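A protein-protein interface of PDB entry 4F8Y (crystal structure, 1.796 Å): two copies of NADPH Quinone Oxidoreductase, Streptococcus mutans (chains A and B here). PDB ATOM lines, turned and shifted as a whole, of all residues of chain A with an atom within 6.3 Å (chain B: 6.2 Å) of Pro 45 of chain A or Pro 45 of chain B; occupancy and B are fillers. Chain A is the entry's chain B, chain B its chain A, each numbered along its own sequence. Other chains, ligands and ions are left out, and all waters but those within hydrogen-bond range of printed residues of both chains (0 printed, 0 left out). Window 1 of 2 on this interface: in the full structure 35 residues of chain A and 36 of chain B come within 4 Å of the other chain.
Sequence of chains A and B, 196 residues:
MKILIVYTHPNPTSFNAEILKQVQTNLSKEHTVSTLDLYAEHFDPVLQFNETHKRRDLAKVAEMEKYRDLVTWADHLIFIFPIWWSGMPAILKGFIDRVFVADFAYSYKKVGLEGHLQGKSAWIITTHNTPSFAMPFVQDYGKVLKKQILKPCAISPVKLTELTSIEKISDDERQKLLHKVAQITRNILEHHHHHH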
ATOM      1  N   TYR A  39      21.058  -1.541  -1.418  1.00  0.00           N
ATOM      2  CA  TYR A  39      19.642  -1.882  -1.479  1.00  0.00           C
ATOM      3  C   TYR A  39      18.819  -0.793  -2.145  1.00  0.00           C
ATOM      4  O   TYR A  39      17.906  -1.091  -2.910  1.00  0.00           O
ATOM      5  CB  TYR A  39      19.086  -2.166  -0.083  1.00  0.00           C
ATOM      6  CG  TYR A  39      19.212  -3.607   0.350  1.00  0.00           C
ATOM      7  CD1 TYR A  39      18.194  -4.518   0.097  1.00  0.00           C
ATOM      8  CD2 TYR A  39      20.349  -4.060   1.009  1.00  0.00           C
ATOM      9  CE1 TYR A  39      18.294  -5.838   0.492  1.00  0.00           C
ATOM     10  CE2 TYR A  39      20.458  -5.384   1.413  1.00  0.00           C
ATOM     11  CZ  TYR A  39      19.425  -6.271   1.148  1.00  0.00           C
ATOM     12  OH  TYR A  39      19.526  -7.592   1.538  1.00  0.00           O
ATOM     13  N   HIS A  42      19.018  -0.642  -5.845  1.00  0.00           N
ATOM     14  CA  HIS A  42      18.546  -1.882  -6.466  1.00  0.00           C
ATOM     15  C   HIS A  42      19.670  -2.579  -7.214  1.00  0.00           C
ATOM     16  O   HIS A  42      19.502  -3.056  -8.335  1.00  0.00           O
ATOM     17  CB  HIS A  42      17.334  -1.627  -7.354  1.00  0.00           C
ATOM     18  CG  HIS A  42      16.220  -0.951  -6.626  1.00  0.00           C
ATOM     19  ND1 HIS A  42      15.419  -1.612  -5.719  1.00  0.00           N
ATOM     20  CD2 HIS A  42      15.808   0.338  -6.625  1.00  0.00           C
ATOM     21  CE1 HIS A  42      14.545  -0.762  -5.210  1.00  0.00           C
ATOM     22  NE2 HIS A  42      14.761   0.427  -5.742  1.00  0.00           N
ATOM     23  N   PHE A  43      20.826  -2.630  -6.561  1.00  0.00           N
ATOM     24  CA  PHE A  43      21.996  -3.257  -7.129  1.00  0.00           C
ATOM     25  C   PHE A  43      21.721  -4.739  -7.417  1.00  0.00           C
ATOM     26  O   PHE A  43      21.174  -5.466  -6.578  1.00  0.00           O
ATOM     27  CB  PHE A  43      23.196  -3.078  -6.192  1.00  0.00           C
ATOM     28  CG  PHE A  43      24.477  -3.625  -6.742  1.00  0.00           C
ATOM     29  CD1 PHE A  43      25.243  -2.872  -7.623  1.00  0.00           C
ATOM     30  CD2 PHE A  43      24.906  -4.898  -6.397  1.00  0.00           C
ATOM     31  CE1 PHE A  43      26.424  -3.375  -8.143  1.00  0.00           C
ATOM     32  CE2 PHE A  43      26.085  -5.415  -6.922  1.00  0.00           C
ATOM     33  CZ  PHE A  43      26.846  -4.651  -7.795  1.00  0.00           C
ATOM     34  N   ASP A  44      22.089  -5.157  -8.625  1.00  0.00           N
ATOM     35  CA  ASP A  44      21.986  -6.541  -9.073  1.00  0.00           C
ATOM     36  C   ASP A  44      23.299  -7.282  -8.786  1.00  0.00           C
ATOM     37  O   ASP A  44      24.326  -7.030  -9.427  1.00  0.00           O
ATOM     38  CB  ASP A  44      21.673  -6.561 -10.566  1.00  0.00           C
ATOM     39  CG  ASP A  44      21.555  -7.961 -11.125  1.00  0.00           C
ATOM     40  OD1 ASP A  44      21.653  -8.944 -10.351  1.00  0.00           O
ATOM     41  OD2 ASP A  44      21.356  -8.068 -12.353  1.00  0.00           O
ATOM     42  N   PRO A  45      23.275  -8.192  -7.804  1.00  0.00           N
ATOM     43  CA  PRO A  45      24.507  -8.828  -7.326  1.00  0.00           C
ATOM     44  C   PRO A  45      24.923 -10.069  -8.116  1.00  0.00           C
ATOM     45  O   PRO A  45      25.954 -10.677  -7.804  1.00  0.00           O
ATOM     46  CB  PRO A  45      24.124  -9.249  -5.909  1.00  0.00           C
ATOM     47  CG  PRO A  45      22.659  -9.547  -6.041  1.00  0.00           C
ATOM     48  CD  PRO A  45      22.148  -8.438  -6.885  1.00  0.00           C
ATOM     49  N   VAL A  46      24.135 -10.450  -9.114  1.00  0.00           N
ATOM     50  CA  VAL A  46      24.389 -11.700  -9.828  1.00  0.00           C
ATOM     51  C   VAL A  46      25.335 -11.522 -11.013  1.00  0.00           C
ATOM     52  O   VAL A  46      24.972 -10.941 -12.029  1.00  0.00           O
ATOM     53  CB  VAL A  46      23.075 -12.363 -10.274  1.00  0.00           C
ATOM     54  CG1 VAL A  46      23.340 -13.735 -10.865  1.00  0.00           C
ATOM     55  CG2 VAL A  46      22.130 -12.466  -9.088  1.00  0.00           C
ATOM     56  N   LEU A  47      26.556 -12.023 -10.850  1.00  0.00           N
ATOM     57  CA  LEU A  47      27.582 -11.975 -11.890  1.00  0.00           C
ATOM     58  C   LEU A  47      27.272 -12.968 -13.011  1.00  0.00           C
ATOM     59  O   LEU A  47      27.024 -14.147 -12.750  1.00  0.00           O
ATOM     60  CB  LEU A  47      28.964 -12.274 -11.294  1.00  0.00           C
ATOM     61  CG  LEU A  47      30.188 -12.340 -12.222  1.00  0.00           C
ATOM     62  CD1 LEU A  47      30.477 -10.988 -12.867  1.00  0.00           C
ATOM     63  CD2 LEU A  47      31.406 -12.837 -11.461  1.00  0.00           C
ATOM     64  N   ALA A  90      24.161 -11.166   0.456  1.00  0.00           N
ATOM     65  CA  ALA A  90      24.334 -11.511  -0.952  1.00  0.00           C
ATOM     66  C   ALA A  90      24.558 -10.307  -1.878  1.00  0.00           C
ATOM     67  O   ALA A  90      25.417 -10.358  -2.765  1.00  0.00           O
ATOM     68  CB  ALA A  90      23.161 -12.368  -1.440  1.00  0.00           C
ATOM     69  N   ILE A  91      23.789  -9.235  -1.679  1.00  0.00           N
ATOM     70  CA  ILE A  91      23.921  -8.029  -2.498  1.00  0.00           C
ATOM     71  C   ILE A  91      25.336  -7.427  -2.420  1.00  0.00           C
ATOM     72  O   ILE A  91      25.841  -6.898  -3.417  1.00  0.00           O
ATOM     73  CB  ILE A  91      22.823  -6.965  -2.167  1.00  0.00           C
ATOM     74  CG1 ILE A  91      22.609  -6.003  -3.341  1.00  0.00           C
ATOM     75  CG2 ILE A  91      23.144  -6.222  -0.881  1.00  0.00           C
ATOM     76  CD1 ILE A  91      21.441  -5.047  -3.141  1.00  0.00           C
ATOM     77  N   LEU A  92      25.975  -7.544  -1.253  1.00  0.00           N
ATOM     78  CA  LEU A  92      27.329  -7.023  -1.034  1.00  0.00           C
ATOM     79  C   LEU A  92      28.404  -7.996  -1.512  1.00  0.00           C
ATOM     80  O   LEU A  92      29.458  -7.572  -2.003  1.00  0.00           O
ATOM     81  CB  LEU A  92      27.558  -6.681   0.439  1.00  0.00           C
ATOM     82  CG  LEU A  92      28.986  -6.228   0.754  1.00  0.00           C
ATOM     83  CD1 LEU A  92      29.311  -4.942  -0.005  1.00  0.00           C
ATOM     84  CD2 LEU A  92      29.203  -6.053   2.252  1.00  0.00           C
ATOM     85  N   LYS A  93      28.144  -9.299  -1.367  1.00  0.00           N
ATOM     86  CA  LYS A  93      29.014 -10.318  -1.960  1.00  0.00           C
ATOM     87  C   LYS A  93      29.096 -10.101  -3.475  1.00  0.00           C
ATOM     88  O   LYS A  93      30.178 -10.139  -4.051  1.00  0.00           O
ATOM     89  CB  LYS A  93      28.514 -11.735  -1.644  1.00  0.00           C
ATOM     90  CG  LYS A  93      29.364 -12.860  -2.251  1.00  0.00           C
ATOM     91  CD  LYS A  93      30.869 -12.637  -2.023  1.00  0.00           C
ATOM     92  CE  LYS A  93      31.683 -13.887  -2.300  1.00  0.00           C
ATOM     93  NZ  LYS A  93      31.426 -14.451  -3.653  1.00  0.00           N
ATOM     94  N   GLY A  94      27.945  -9.846  -4.099  1.00  0.00           N
ATOM     95  CA  GLY A  94      27.864  -9.631  -5.532  1.00  0.00           C
ATOM     96  C   GLY A  94      28.391  -8.283  -5.998  1.00  0.00           C
ATOM     97  O   GLY A  94      28.743  -8.121  -7.168  1.00  0.00           O
ATOM     98  N   PHE A  95      28.428  -7.305  -5.096  1.00  0.00           N
ATOM     99  CA  PHE A  95      29.084  -6.040  -5.396  1.00  0.00           C
ATOM    100  C   PHE A  95      30.562  -6.318  -5.667  1.00  0.00           C
ATOM    101  O   PHE A  95      31.134  -5.820  -6.635  1.00  0.00           O
ATOM    102  CB  PHE A  95      28.903  -5.053  -4.234  1.00  0.00           C
ATOM    103  CG  PHE A  95      29.686  -3.763  -4.381  1.00  0.00           C
ATOM    104  CD1 PHE A  95      29.270  -2.776  -5.262  1.00  0.00           C
ATOM    105  CD2 PHE A  95      30.819  -3.530  -3.609  1.00  0.00           C
ATOM    106  CE1 PHE A  95      29.983  -1.587  -5.381  1.00  0.00           C
ATOM    107  CE2 PHE A  95      31.538  -2.349  -3.728  1.00  0.00           C
ATOM    108  CZ  PHE A  95      31.122  -1.378  -4.611  1.00  0.00           C
ATOM    109  N   ASP A  97      31.900  -9.489  -6.335  1.00  0.00           N
ATOM    110  CA  ASP A  97      31.906 -10.378  -7.494  1.00  0.00           C
ATOM    111  C   ASP A  97      31.923  -9.593  -8.803  1.00  0.00           C
ATOM    112  O   ASP A  97      32.722  -9.878  -9.697  1.00  0.00           O
ATOM    113  CB  ASP A  97      30.670 -11.284  -7.489  1.00  0.00           C
ATOM    114  CG  ASP A  97      30.697 -12.340  -6.387  1.00  0.00           C
ATOM    115  OD1 ASP A  97      31.760 -12.573  -5.771  1.00  0.00           O
ATOM    116  OD2 ASP A  97      29.628 -12.954  -6.151  1.00  0.00           O
ATOM    117  N   ARG A  98      31.040  -8.601  -8.908  1.00  0.00           N
ATOM    118  CA  ARG A  98      30.795  -7.908 -10.169  1.00  0.00           C
ATOM    119  C   ARG A  98      31.688  -6.690 -10.413  1.00  0.00           C
ATOM    120  O   ARG A  98      32.001  -6.371 -11.562  1.00  0.00           O
ATOM    121  CB  ARG A  98      29.321  -7.497 -10.272  1.00  0.00           C
ATOM    122  CG  ARG A  98      28.329  -8.663 -10.277  1.00  0.00           C
ATOM    123  CD  ARG A  98      26.961  -8.209 -10.799  1.00  0.00           C
ATOM    124  NE  ARG A  98      27.033  -7.764 -12.189  1.00  0.00           N
ATOM    125  CZ  ARG A  98      26.071  -7.098 -12.815  1.00  0.00           C
ATOM    126  NH1 ARG A  98      24.949  -6.785 -12.179  1.00  0.00           N
ATOM    127  NH2 ARG A  98      26.233  -6.733 -14.080  1.00  0.00           N
ATOM    128  N   TYR B  39      20.889 -20.171 -11.513  1.00  0.00           N
ATOM    129  CA  TYR B  39      21.048 -19.224 -12.618  1.00  0.00           C
ATOM    130  C   TYR B  39      19.952 -19.365 -13.674  1.00  0.00           C
ATOM    131  O   TYR B  39      19.433 -18.372 -14.185  1.00  0.00           O
ATOM    132  CB  TYR B  39      22.440 -19.354 -13.251  1.00  0.00           C
ATOM    133  CG  TYR B  39      23.477 -18.447 -12.619  1.00  0.00           C
ATOM    134  CD1 TYR B  39      23.659 -17.153 -13.084  1.00  0.00           C
ATOM    135  CD2 TYR B  39      24.263 -18.879 -11.555  1.00  0.00           C
ATOM    136  CE1 TYR B  39      24.594 -16.311 -12.512  1.00  0.00           C
ATOM    137  CE2 TYR B  39      25.204 -18.050 -10.979  1.00  0.00           C
ATOM    138  CZ  TYR B  39      25.364 -16.760 -11.461  1.00  0.00           C
ATOM    139  OH  TYR B  39      26.297 -15.908 -10.903  1.00  0.00           O
ATOM    140  N   HIS B  42      16.754 -17.880 -12.557  1.00  0.00           N
ATOM    141  CA  HIS B  42      16.829 -16.430 -12.372  1.00  0.00           C
ATOM    142  C   HIS B  42      16.594 -16.090 -10.900  1.00  0.00           C
ATOM    143  O   HIS B  42      15.913 -15.106 -10.572  1.00  0.00           O
ATOM    144  CB  HIS B  42      15.806 -15.685 -13.239  1.00  0.00           C
ATOM    145  CG  HIS B  42      15.503 -16.354 -14.547  1.00  0.00           C
ATOM    146  ND1 HIS B  42      16.428 -16.460 -15.565  1.00  0.00           N
ATOM    147  CD2 HIS B  42      14.366 -16.931 -15.009  1.00  0.00           C
ATOM    148  CE1 HIS B  42      15.877 -17.087 -16.591  1.00  0.00           C
ATOM    149  NE2 HIS B  42      14.627 -17.379 -16.282  1.00  0.00           N
ATOM    150  N   PHE B  43      17.155 -16.913 -10.016  1.00  0.00           N
ATOM    151  CA  PHE B  43      16.979 -16.741  -8.577  1.00  0.00           C
ATOM    152  C   PHE B  43      17.402 -15.345  -8.121  1.00  0.00           C
ATOM    153  O   PHE B  43      18.489 -14.861  -8.458  1.00  0.00           O
ATOM    154  CB  PHE B  43      17.741 -17.815  -7.798  1.00  0.00           C
ATOM    155  CG  PHE B  43      17.444 -17.819  -6.324  1.00  0.00           C
ATOM    156  CD1 PHE B  43      16.271 -18.369  -5.844  1.00  0.00           C
ATOM    157  CD2 PHE B  43      18.343 -17.279  -5.416  1.00  0.00           C
ATOM    158  CE1 PHE B  43      15.989 -18.368  -4.478  1.00  0.00           C
ATOM    159  CE2 PHE B  43      18.072 -17.273  -4.060  1.00  0.00           C
ATOM    160  CZ  PHE B  43      16.895 -17.820  -3.588  1.00  0.00           C
ATOM    161  N   ASP B  44      16.510 -14.705  -7.367  1.00  0.00           N
ATOM    162  CA  ASP B  44      16.762 -13.405  -6.756  1.00  0.00           C
ATOM    163  C   ASP B  44      17.358 -13.621  -5.361  1.00  0.00           C
ATOM    164  O   ASP B  44      16.635 -13.983  -4.427  1.00  0.00           O
ATOM    165  CB  ASP B  44      15.445 -12.619  -6.677  1.00  0.00           C
ATOM    166  CG  ASP B  44      15.622 -11.197  -6.154  1.00  0.00           C
ATOM    167  OD1 ASP B  44      16.751 -10.811  -5.776  1.00  0.00           O
ATOM    168  OD2 ASP B  44      14.613 -10.461  -6.113  1.00  0.00           O
ATOM    169  N   PRO B  45      18.682 -13.400  -5.218  1.00  0.00           N
ATOM    170  CA  PRO B  45      19.378 -13.684  -3.963  1.00  0.00           C
ATOM    171  C   PRO B  45      19.286 -12.561  -2.928  1.00  0.00           C
ATOM    172  O   PRO B  45      19.924 -12.676  -1.881  1.00  0.00           O
ATOM    173  CB  PRO B  45      20.829 -13.841  -4.417  1.00  0.00           C
ATOM    174  CG  PRO B  45      20.959 -12.919  -5.576  1.00  0.00           C
ATOM    175  CD  PRO B  45      19.603 -12.868  -6.244  1.00  0.00           C
ATOM    176  N   VAL B  46      18.515 -11.506  -3.202  1.00  0.00           N
ATOM    177  CA  VAL B  46      18.460 -10.338  -2.305  1.00  0.00           C
ATOM    178  C   VAL B  46      17.368 -10.440  -1.224  1.00  0.00           C
ATOM    179  O   VAL B  46      16.191 -10.235  -1.496  1.00  0.00           O
ATOM    180  CB  VAL B  46      18.317  -9.001  -3.088  1.00  0.00           C
ATOM    181  CG1 VAL B  46      18.353  -7.814  -2.133  1.00  0.00           C
ATOM    182  CG2 VAL B  46      19.411  -8.863  -4.131  1.00  0.00           C
ATOM    183  N   LEU B  47      17.781 -10.758  -0.002  1.00  0.00           N
ATOM    184  CA  LEU B  47      16.866 -10.893   1.130  1.00  0.00           C
ATOM    185  C   LEU B  47      16.306  -9.534   1.567  1.00  0.00           C
ATOM    186  O   LEU B  47      17.059  -8.607   1.901  1.00  0.00           O
ATOM    187  CB  LEU B  47      17.586 -11.580   2.305  1.00  0.00           C
ATOM    188  CG  LEU B  47      16.876 -11.816   3.647  1.00  0.00           C
ATOM    189  CD1 LEU B  47      15.845 -12.931   3.549  1.00  0.00           C
ATOM    190  CD2 LEU B  47      17.900 -12.139   4.730  1.00  0.00           C
ATOM    191  N   ALA B  90      27.510 -14.891  -5.119  1.00  0.00           N
ATOM    192  CA  ALA B  90      26.441 -14.098  -4.530  1.00  0.00           C
ATOM    193  C   ALA B  90      25.062 -14.761  -4.616  1.00  0.00           C
ATOM    194  O   ALA B  90      24.301 -14.715  -3.643  1.00  0.00           O
ATOM    195  CB  ALA B  90      26.401 -12.708  -5.153  1.00  0.00           C
ATOM    196  N   ILE B  91      24.734 -15.361  -5.769  1.00  0.00           N
ATOM    197  CA  ILE B  91      23.396 -15.933  -5.986  1.00  0.00           C
ATOM    198  C   ILE B  91      23.121 -17.139  -5.086  1.00  0.00           C
ATOM    199  O   ILE B  91      21.989 -17.354  -4.652  1.00  0.00           O
ATOM    200  CB  ILE B  91      23.148 -16.312  -7.467  1.00  0.00           C
ATOM    201  CG1 ILE B  91      21.644 -16.476  -7.740  1.00  0.00           C
ATOM    202  CG2 ILE B  91      23.910 -17.573  -7.828  1.00  0.00           C
ATOM    203  CD1 ILE B  91      21.286 -16.608  -9.215  1.00  0.00           C
ATOM    204  N   LEU B  92      24.159 -17.925  -4.805  1.00  0.00           N
ATOM    205  CA  LEU B  92      24.029 -19.052  -3.879  1.00  0.00           C
ATOM    206  C   LEU B  92      24.034 -18.575  -2.424  1.00  0.00           C
ATOM    207  O   LEU B  92      23.307 -19.129  -1.591  1.00  0.00           O
ATOM    208  CB  LEU B  92      25.127 -20.101  -4.092  1.00  0.00           C
ATOM    209  CG  LEU B  92      25.126 -21.229  -3.050  1.00  0.00           C
ATOM    210  CD1 LEU B  92      23.924 -22.149  -3.236  1.00  0.00           C
ATOM    211  CD2 LEU B  92      26.427 -22.024  -3.069  1.00  0.00           C
ATOM    212  N   LYS B  93      24.855 -17.563  -2.117  1.00  0.00           N
ATOM    213  CA  LYS B  93      24.847 -16.953  -0.783  1.00  0.00           C
ATOM    214  C   LYS B  93      23.449 -16.414  -0.437  1.00  0.00           C
ATOM    215  O   LYS B  93      22.977 -16.554   0.689  1.00  0.00           O
ATOM    216  CB  LYS B  93      25.906 -15.856  -0.679  1.00  0.00           C
ATOM    217  CG  LYS B  93      25.914 -15.084   0.640  1.00  0.00           C
ATOM    218  CD  LYS B  93      25.863 -16.012   1.846  1.00  0.00           C
ATOM    219  CE  LYS B  93      26.233 -15.284   3.125  1.00  0.00           C
ATOM    220  NZ  LYS B  93      25.284 -14.185   3.463  1.00  0.00           N
ATOM    221  N   GLY B  94      22.781 -15.820  -1.419  1.00  0.00           N
ATOM    222  CA  GLY B  94      21.418 -15.362  -1.249  1.00  0.00           C
ATOM    223  C   GLY B  94      20.414 -16.498  -1.161  1.00  0.00           C
ATOM    224  O   GLY B  94      19.355 -16.343  -0.544  1.00  0.00           O
ATOM    225  N   PHE B  95      20.735 -17.634  -1.771  1.00  0.00           N
ATOM    226  CA  PHE B  95      19.908 -18.841  -1.625  1.00  0.00           C
ATOM    227  C   PHE B  95      19.803 -19.246  -0.144  1.00  0.00           C
ATOM    228  O   PHE B  95      18.717 -19.524   0.371  1.00  0.00           O
ATOM    229  CB  PHE B  95      20.463 -19.996  -2.481  1.00  0.00           C
ATOM    230  CG  PHE B  95      19.759 -21.315  -2.258  1.00  0.00           C
ATOM    231  CD1 PHE B  95      18.487 -21.536  -2.777  1.00  0.00           C
ATOM    232  CD2 PHE B  95      20.371 -22.328  -1.524  1.00  0.00           C
ATOM    233  CE1 PHE B  95      17.835 -22.743  -2.571  1.00  0.00           C
ATOM    234  CE2 PHE B  95      19.725 -23.537  -1.303  1.00  0.00           C
ATOM    235  CZ  PHE B  95      18.454 -23.746  -1.829  1.00  0.00           C
ATOM    236  N   ASP B  97      20.639 -17.136   2.516  1.00  0.00           N
ATOM    237  CA  ASP B  97      20.022 -15.999   3.197  1.00  0.00           C
ATOM    238  C   ASP B  97      18.496 -16.063   3.152  1.00  0.00           C
ATOM    239  O   ASP B  97      17.823 -15.854   4.161  1.00  0.00           O
ATOM    240  CB  ASP B  97      20.441 -14.667   2.566  1.00  0.00           C
ATOM    241  CG  ASP B  97      21.898 -14.337   2.768  1.00  0.00           C
ATOM    242  OD1 ASP B  97      22.574 -14.993   3.590  1.00  0.00           O
ATOM    243  OD2 ASP B  97      22.360 -13.401   2.089  1.00  0.00           O
ATOM    244  N   ARG B  98      17.943 -16.325   1.975  1.00  0.00           N
ATOM    245  CA  ARG B  98      16.499 -16.212   1.799  1.00  0.00           C
ATOM    246  C   ARG B  98      15.720 -17.477   2.149  1.00  0.00           C
ATOM    247  O   ARG B  98      14.586 -17.392   2.620  1.00  0.00           O
ATOM    248  CB  ARG B  98      16.169 -15.768   0.380  1.00  0.00           C
ATOM    249  CG  ARG B  98      16.734 -14.422   0.022  1.00  0.00           C
ATOM    250  CD  ARG B  98      16.125 -13.975  -1.271  1.00  0.00           C
ATOM    251  NE  ARG B  98      14.682 -13.794  -1.138  1.00  0.00           N
ATOM    252  CZ  ARG B  98      13.889 -13.434  -2.139  1.00  0.00           C
ATOM    253  NH1 ARG B  98      14.402 -13.236  -3.345  1.00  0.00           N
ATOM    254  NH2 ARG B  98      12.587 -13.284  -1.939  1.00  0.00           N
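Pro 45 of chain A touches three residues of chain B. Of chain A, only Pro 45, Val 46 and Ala 90 come within 4 Å of Pro 45 of chain B. Printed residues of chain B within 4 Å of Lys 93 of chain A: Ala 90 (3.9 Å). Of the printed residues of chain A, Tyr 39 of chain B touches Val 46 (3.3 Å) and Leu 47 (2.7 Å). Printed residues of chain B within 4 Å of Asp 97 of chain A: Ala 90. Of the printed residues of chain B, Tyr 39 of chain A touches Val 46 (3.3 Å) and Leu 47 (2.7 Å). Of the printed residues of chain A, Gly 94 of chain B touches Ala 90 (3.5 Å). Phe 43 of chain A touches none of the printed residues of chain B.
OD2 of Asp 97 of chain A sits at hydrogen-bond distance from N of Ala 90 of chain B. O of Leu 47 of chain A sits at hydrogen-bond distance from OH of Tyr 39 of chain B (2.7 Å). The backbone carbonyl oxygen (O) of Leu 47 of chain B sits at hydrogen-bond distance from the side-chain hydroxyl (OH) of Tyr 39 of chain A (2.7 Å). The backbone NH of Ala 90 of chain A sits at hydrogen-bond distance from the side-chain carboxylate of Asp 97 of chain B.
Tyr 39 of chain A touches Val 46 of chain B, and with the chains exchanged Val 46 of chain A touches Tyr 39 of chain B. Pro 45 of chain A touches Val 46 of chain B, and with the chains exchanged Val 46 of chain A touches Pro 45 of chain B. Pro 45 of chain A touches Ala 90 of chain B, and with the chains exchanged Ala 90 of chain A touches Pro 45 of chain B. Ala 90 of chain A touches Gly 94 of chain B, and with the chains exchanged Gly 94 of chain A touches Ala 90 of chain B. 15 positions are printed for both chains.
Hydrophobic or aromatic side chains of chain A within 4 Å of the printed part of chain B: Tyr 39, Pro 45, Val 46 and Ala 90. Along chain A the printed residues that touch a printed residue of chain B span positions 39 to 97. Printed residues of chain B that touch a printed residue of chain A: Tyr 39, Pro 45, Val 46, Leu 47, Ala 90, Ile 91, Gly 94 and Asp 97. Hydrophobic or aromatic side chains of chain B that line the printed part of chain A: Tyr 39, Pro 45, Val 46, Ala 90 and Ile 91. Among the printed residues, 16 pairs touch across the chains. Among the printed residues, no Asp or Glu carboxylate lies within 4 Å of a Lys or Arg side-chain nitrogen of the other chain.
The side-chain carboxylate (OD1) of Asp 44 of chain A lies within hydrogen-bond range of the backbone NH (N) of Val 46 of chain A. The side-chain amino group (NZ) of Lys 93 of chain B is in salt-bridge range of the side-chain carboxylate (OD1) of Asp 97 of chain B (2.8 Å). The side-chain amino group of Lys 93 of chain A is in salt-bridge range of the side-chain carboxylate of Asp 97 of chain A (2.9 Å). The backbone NH of Val 46 of chain B sits at hydrogen-bond distance from the side-chain carboxylate of Asp 44 of chain B (3.2 Å).
Among the printed residues, merely in contact across the chains: Tyr 39 of chain A with Val 46 of chain B (3.3 Å), Pro 45 of chain A with Pro 45 of chain B (3.8 Å), Pro 45 of chain A with Val 46 of chain B (3.8 Å), Pro 45 of chain A with Ala 90 of chain B (3.4 Å), Val 46 of chain A with Tyr 39 of chain B (3.3 Å), Val 46 of chain A with Pro 45 of chain B (3.7 Å), Val 46 of chain A with Ile 91 of chain B (3.9 Å), Ala 90 of chain A with Pro 45 of chain B (3.3 Å), Ala 90 of chain A with Ala 90 of chain B (3.4 Å), Ala 90 of chain A with Gly 94 of chain B (3.5 Å), Lys 93 of chain A with Ala 90 of chain B (3.9 Å) and Gly 94 of chain A with Ala 90 of chain B (3.4 Å).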
